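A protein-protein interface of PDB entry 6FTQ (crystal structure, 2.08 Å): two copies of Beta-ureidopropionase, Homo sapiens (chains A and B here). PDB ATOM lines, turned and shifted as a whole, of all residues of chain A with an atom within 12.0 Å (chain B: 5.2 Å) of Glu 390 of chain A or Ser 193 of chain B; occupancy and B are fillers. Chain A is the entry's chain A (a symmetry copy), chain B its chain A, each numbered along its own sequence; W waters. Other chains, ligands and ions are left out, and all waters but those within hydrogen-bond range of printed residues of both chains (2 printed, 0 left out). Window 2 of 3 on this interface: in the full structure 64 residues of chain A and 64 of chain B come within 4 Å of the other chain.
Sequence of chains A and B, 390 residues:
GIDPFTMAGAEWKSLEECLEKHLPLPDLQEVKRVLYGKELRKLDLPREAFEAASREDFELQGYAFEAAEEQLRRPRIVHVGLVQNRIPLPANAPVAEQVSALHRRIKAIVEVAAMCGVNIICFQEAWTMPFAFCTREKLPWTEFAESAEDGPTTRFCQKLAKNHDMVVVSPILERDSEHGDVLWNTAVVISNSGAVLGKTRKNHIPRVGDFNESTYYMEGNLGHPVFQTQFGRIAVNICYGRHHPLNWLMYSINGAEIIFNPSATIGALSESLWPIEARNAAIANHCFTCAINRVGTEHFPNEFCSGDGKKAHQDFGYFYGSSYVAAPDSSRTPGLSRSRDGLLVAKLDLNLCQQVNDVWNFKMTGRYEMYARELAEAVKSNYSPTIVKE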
ATOM      1  N   THR A 386      40.485  18.488   7.176  1.00  0.00           N
ATOM      2  CA  THR A 386      39.158  18.357   7.819  1.00  0.00           C
ATOM      3  C   THR A 386      38.210  17.503   6.943  1.00  0.00           C
ATOM      4  O   THR A 386      37.402  18.047   6.182  1.00  0.00           O
ATOM      5  CB  THR A 386      38.542  19.778   8.100  1.00  0.00           C
ATOM      6  OG1 THR A 386      39.492  20.573   8.826  1.00  0.00           O
ATOM      7  CG2 THR A 386      37.252  19.707   8.925  1.00  0.00           C
ATOM      8  N   ILE A 387      38.317  16.172   7.070  1.00  0.00           N
ATOM      9  CA  ILE A 387      37.562  15.233   6.211  1.00  0.00           C
ATOM     10  C   ILE A 387      36.730  14.213   7.003  1.00  0.00           C
ATOM     11  O   ILE A 387      37.253  13.490   7.854  1.00  0.00           O
ATOM     12  CB  ILE A 387      38.460  14.521   5.158  1.00  0.00           C
ATOM     13  CG1 ILE A 387      37.581  13.793   4.121  1.00  0.00           C
ATOM     14  CG2 ILE A 387      39.452  13.554   5.808  1.00  0.00           C
ATOM     15  CD1 ILE A 387      38.342  13.191   2.957  1.00  0.00           C
ATOM     16  N   VAL A 388      35.437  14.149   6.673  1.00  0.00           N
ATOM     17  CA  VAL A 388      34.462  13.312   7.368  1.00  0.00           C
ATOM     18  C   VAL A 388      34.131  12.064   6.521  1.00  0.00           C
ATOM     19  O   VAL A 388      33.897  12.159   5.314  1.00  0.00           O
ATOM     20  CB  VAL A 388      33.170  14.109   7.676  1.00  0.00           C
ATOM     21  CG1 VAL A 388      32.323  13.370   8.708  1.00  0.00           C
ATOM     22  CG2 VAL A 388      33.487  15.525   8.156  1.00  0.00           C
ATOM     23  N   LYS A 389      34.117  10.901   7.177  1.00  0.00           N
ATOM     24  CA  LYS A 389      33.886   9.612   6.522  1.00  0.00           C
ATOM     25  C   LYS A 389      32.837   8.806   7.311  1.00  0.00           C
ATOM     26  O   LYS A 389      32.583   9.095   8.486  1.00  0.00           O
ATOM     27  CB  LYS A 389      35.217   8.847   6.409  1.00  0.00           C
ATOM     28  CG  LYS A 389      35.271   7.845   5.260  1.00  0.00           C
ATOM     29  CD  LYS A 389      36.634   7.174   5.144  1.00  0.00           C
ATOM     30  CE  LYS A 389      36.662   6.143   4.021  1.00  0.00           C
ATOM     31  NZ  LYS A 389      35.787   4.962   4.280  1.00  0.00           N
ATOM     32  N   GLU A 390      32.213   7.822   6.660  1.00  0.00           N
ATOM     33  CA  GLU A 390      31.209   6.972   7.312  1.00  0.00           C
ATOM     34  C   GLU A 390      31.893   5.941   8.219  1.00  0.00           C
ATOM     35  O   GLU A 390      33.084   5.676   8.095  1.00  0.00           O
ATOM     36  CB  GLU A 390      30.316   6.260   6.279  1.00  0.00           C
ATOM     37  CG  GLU A 390      28.968   5.820   6.846  1.00  0.00           C
ATOM     38  CD  GLU A 390      28.058   5.146   5.834  1.00  0.00           C
ATOM     39  OE1 GLU A 390      28.005   5.578   4.665  1.00  0.00           O
ATOM     40  OE2 GLU A 390      27.375   4.178   6.224  1.00  0.00           O
ATOM     41  OXT GLU A 390      31.281   5.344   9.101  1.00  0.00           O
ATOM     42  N   LYS B 162      18.887   5.967   0.980  1.00  0.00           N
ATOM     43  CA  LYS B 162      19.007   4.521   0.994  1.00  0.00           C
ATOM     44  C   LYS B 162      18.210   3.903  -0.152  1.00  0.00           C
ATOM     45  O   LYS B 162      18.705   3.030  -0.849  1.00  0.00           O
ATOM     46  CB  LYS B 162      18.517   3.958   2.337  1.00  0.00           C
ATOM     47  CG  LYS B 162      18.908   2.518   2.616  1.00  0.00           C
ATOM     48  CD  LYS B 162      18.472   2.134   4.032  1.00  0.00           C
ATOM     49  CE  LYS B 162      18.181   0.654   4.181  1.00  0.00           C
ATOM     50  NZ  LYS B 162      19.418  -0.160   4.094  1.00  0.00           N
ATOM     51  N   ASP B 165      20.035   4.649  -3.490  1.00  0.00           N
ATOM     52  CA  ASP B 165      21.496   4.558  -3.469  1.00  0.00           C
ATOM     53  C   ASP B 165      22.173   5.908  -3.847  1.00  0.00           C
ATOM     54  O   ASP B 165      23.107   5.965  -4.666  1.00  0.00           O
ATOM     55  CB  ASP B 165      21.973   3.407  -4.385  1.00  0.00           C
ATOM     56  CG  ASP B 165      23.419   3.024  -4.124  1.00  0.00           C
ATOM     57  OD1 ASP B 165      23.879   3.227  -2.994  1.00  0.00           O
ATOM     58  OD2 ASP B 165      24.101   2.515  -5.041  1.00  0.00           O
ATOM     59  N   SER B 191      24.651   9.867   3.521  1.00  0.00           N
ATOM     60  CA  SER B 191      25.268   8.862   2.680  1.00  0.00           C
ATOM     61  C   SER B 191      24.236   8.080   1.881  1.00  0.00           C
ATOM     62  O   SER B 191      23.076   7.974   2.290  1.00  0.00           O
ATOM     63  CB  SER B 191      26.051   7.875   3.535  1.00  0.00           C
ATOM     64  OG  SER B 191      26.472   6.781   2.765  1.00  0.00           O
ATOM     65  N   ASN B 192      24.686   7.492   0.774  1.00  0.00           N
ATOM     66  CA  ASN B 192      23.873   6.567  -0.009  1.00  0.00           C
ATOM     67  C   ASN B 192      23.468   5.285   0.749  1.00  0.00           C
ATOM     68  O   ASN B 192      22.546   4.595   0.311  1.00  0.00           O
ATOM     69  CB  ASN B 192      24.537   6.214  -1.357  1.00  0.00           C
ATOM     70  CG  ASN B 192      25.901   5.584  -1.208  1.00  0.00           C
ATOM     71  OD1 ASN B 192      26.774   6.141  -0.543  1.00  0.00           O
ATOM     72  ND2 ASN B 192      26.112   4.442  -1.862  1.00  0.00           N
ATOM     73  N   SER B 193      24.120   4.978   1.871  1.00  0.00           N
ATOM     74  CA  SER B 193      23.645   3.914   2.770  1.00  0.00           C
ATOM     75  C   SER B 193      22.515   4.345   3.705  1.00  0.00           C
ATOM     76  O   SER B 193      22.003   3.516   4.449  1.00  0.00           O
ATOM     77  CB  SER B 193      24.798   3.400   3.634  1.00  0.00           C
ATOM     78  OG  SER B 193      25.169   4.410   4.577  1.00  0.00           O
ATOM     79  N   GLY B 194      22.162   5.629   3.718  1.00  0.00           N
ATOM     80  CA  GLY B 194      21.173   6.160   4.657  1.00  0.00           C
ATOM     81  C   GLY B 194      21.733   6.707   5.966  1.00  0.00           C
ATOM     82  O   GLY B 194      20.984   7.303   6.744  1.00  0.00           O
ATOM     83  N   ALA B 195      23.035   6.527   6.208  1.00  0.00           N
ATOM     84  CA  ALA B 195      23.687   7.033   7.411  1.00  0.00           C
ATOM     85  C   ALA B 195      23.987   8.531   7.264  1.00  0.00           C
ATOM     86  O   ALA B 195      24.343   9.012   6.175  1.00  0.00           O
ATOM     87  CB  ALA B 195      24.972   6.261   7.687  1.00  0.00           C
ATOM     88  N   LEU B 197      26.306  11.457   7.476  1.00  0.00           N
ATOM     89  CA  LEU B 197      27.766  11.626   7.482  1.00  0.00           C
ATOM     90  C   LEU B 197      28.191  12.768   8.398  1.00  0.00           C
ATOM     91  O   LEU B 197      29.206  12.660   9.073  1.00  0.00           O
ATOM     92  CB  LEU B 197      28.336  11.835   6.074  1.00  0.00           C
ATOM     93  CG  LEU B 197      28.308  10.622   5.149  1.00  0.00           C
ATOM     94  CD1 LEU B 197      28.894  10.991   3.799  1.00  0.00           C
ATOM     95  CD2 LEU B 197      29.058   9.432   5.738  1.00  0.00           C
ATOM     96  N   GLN B 228      33.867  12.731   2.525  1.00  0.00           N
ATOM     97  CA  GLN B 228      34.270  11.665   1.624  1.00  0.00           C
ATOM     98  C   GLN B 228      33.084  10.738   1.387  1.00  0.00           C
ATOM     99  O   GLN B 228      32.600  10.142   2.318  1.00  0.00           O
ATOM    100  CB  GLN B 228      35.435  10.877   2.219  1.00  0.00           C
ATOM    101  CG  GLN B 228      36.143   9.992   1.195  1.00  0.00           C
ATOM    102  CD  GLN B 228      37.574   9.685   1.599  1.00  0.00           C
ATOM    103  OE1 GLN B 228      38.508  10.417   1.217  1.00  0.00           O
ATOM    104  NE2 GLN B 228      37.757   8.629   2.396  1.00  0.00           N
HETATM  105  O   HOH W   1      30.409  10.226   9.846  1.00  0.00           O
HETATM  106  O   HOH W   2      32.198   8.129   3.924  1.00  0.00           O
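No position is printed for both chains.
The side-chain hydroxyl (OG) of Ser 191 of chain B sits at hydrogen-bond distance from the side-chain amide oxygen (OD1) of Asn 192 of chain B.
OG of Ser 191 of chain B is in hydrogen-bond range of N of Ser 193 of chain B.
N of Ala 195 of chain B lies close to OG of Ser 193 of chain B (3.4 Å).
The side-chain carboxylate of Glu 390 of chain A sits at hydrogen-bond distance from the side-chain hydroxyl of Ser 191 of chain B (2.7 Å).
OE2 of Glu 390 of chain A sits at hydrogen-bond distance from OG of Ser 193 of chain B, at 2.8 Å.
The backbone NH of Gln 228 of chain B lies within hydrogen-bond range of the backbone carbonyl oxygen of Val 388 of chain A (2.8 Å).
Of the 5 printed residues of chain A, 4 touch a printed residue of chain B.
Printed residues of chain A that touch a printed residue of chain B: Ile 387, Val 388, Lys 389 and Glu 390.
Hydrophobic or aromatic side chains of chain A that line the printed part of chain B: Ile 387 and Val 388.
Of the 9 printed residues of chain B, 5 touch a printed residue of chain A.
Glu 390 of chain A touches four residues of chain B.
Ser 193 of chain B touches one residue of chain A.
No residue of chain A comes within 4 Å of Lys 162 of chain B.
Asp 165 of chain B touches none of the printed residues of chain A.
Of chain A, only Glu 390 (2.7 Å) comes within 4 Å of Ser 191 of chain B.
No residue of chain A comes within 4 Å of Asn 192 of chain B.
No residue of chain A comes within 4 Å of Gly 194 of chain B.
Ala 195 of chain B touches just one residue of chain A: Glu 390.
Of chain A, only Val 388 (3.2 Å) and Glu 390 (3.5 Å) come within 4 Å of Leu 197 of chain B.
Printed residues of chain B within 4 Å of Lys 389 of chain A: Gln 228 (3.2 Å).
Of the printed residues of chain B, Val 388 of chain A touches Leu 197 and Gln 228.
Printed residues of chain A within 4 Å of Gln 228 of chain B: Ile 387 (3.3 Å), Val 388 (2.8 Å) and Lys 389 (3.2 Å).
Of the printed residues of chain B, Ile 387 of chain A touches Gln 228 (3.3 Å).
Thr 386 of chain A touches none of the printed residues of chain B.
The nearest residue of chain B that does not touch Glu 390 of chain A is Gln 228 of chain B (4.9 Å).
The nearest printed residue of chain B that does not touch Val 388 of chain A is Ser 191 of chain B (9.1 Å).
Ile 387 of chain A touches Gln 228 of chain B.
Val 388 of chain A touches Leu 197 of chain B (CG1 to O, 3.2 Å).
Gln 228 of chain B touches Lys 389 of chain A.
Ala 195 of chain B touches Glu 390 of chain A.
CD2 of Leu 197 of chain B touches CB of Glu 390 of chain A (3.5 Å).
Water W2 bridges the backbone carbonyl oxygen (O) of Gln 228 of chain B (2.6 Å) and the backbone NH (N) of Glu 390 of chain A (2.8 Å).
Water W1 lies within hydrogen-bond range of O of Lys 389 of chain A (2.8 Å) and O of Leu 197 of chain B (2.8 Å).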
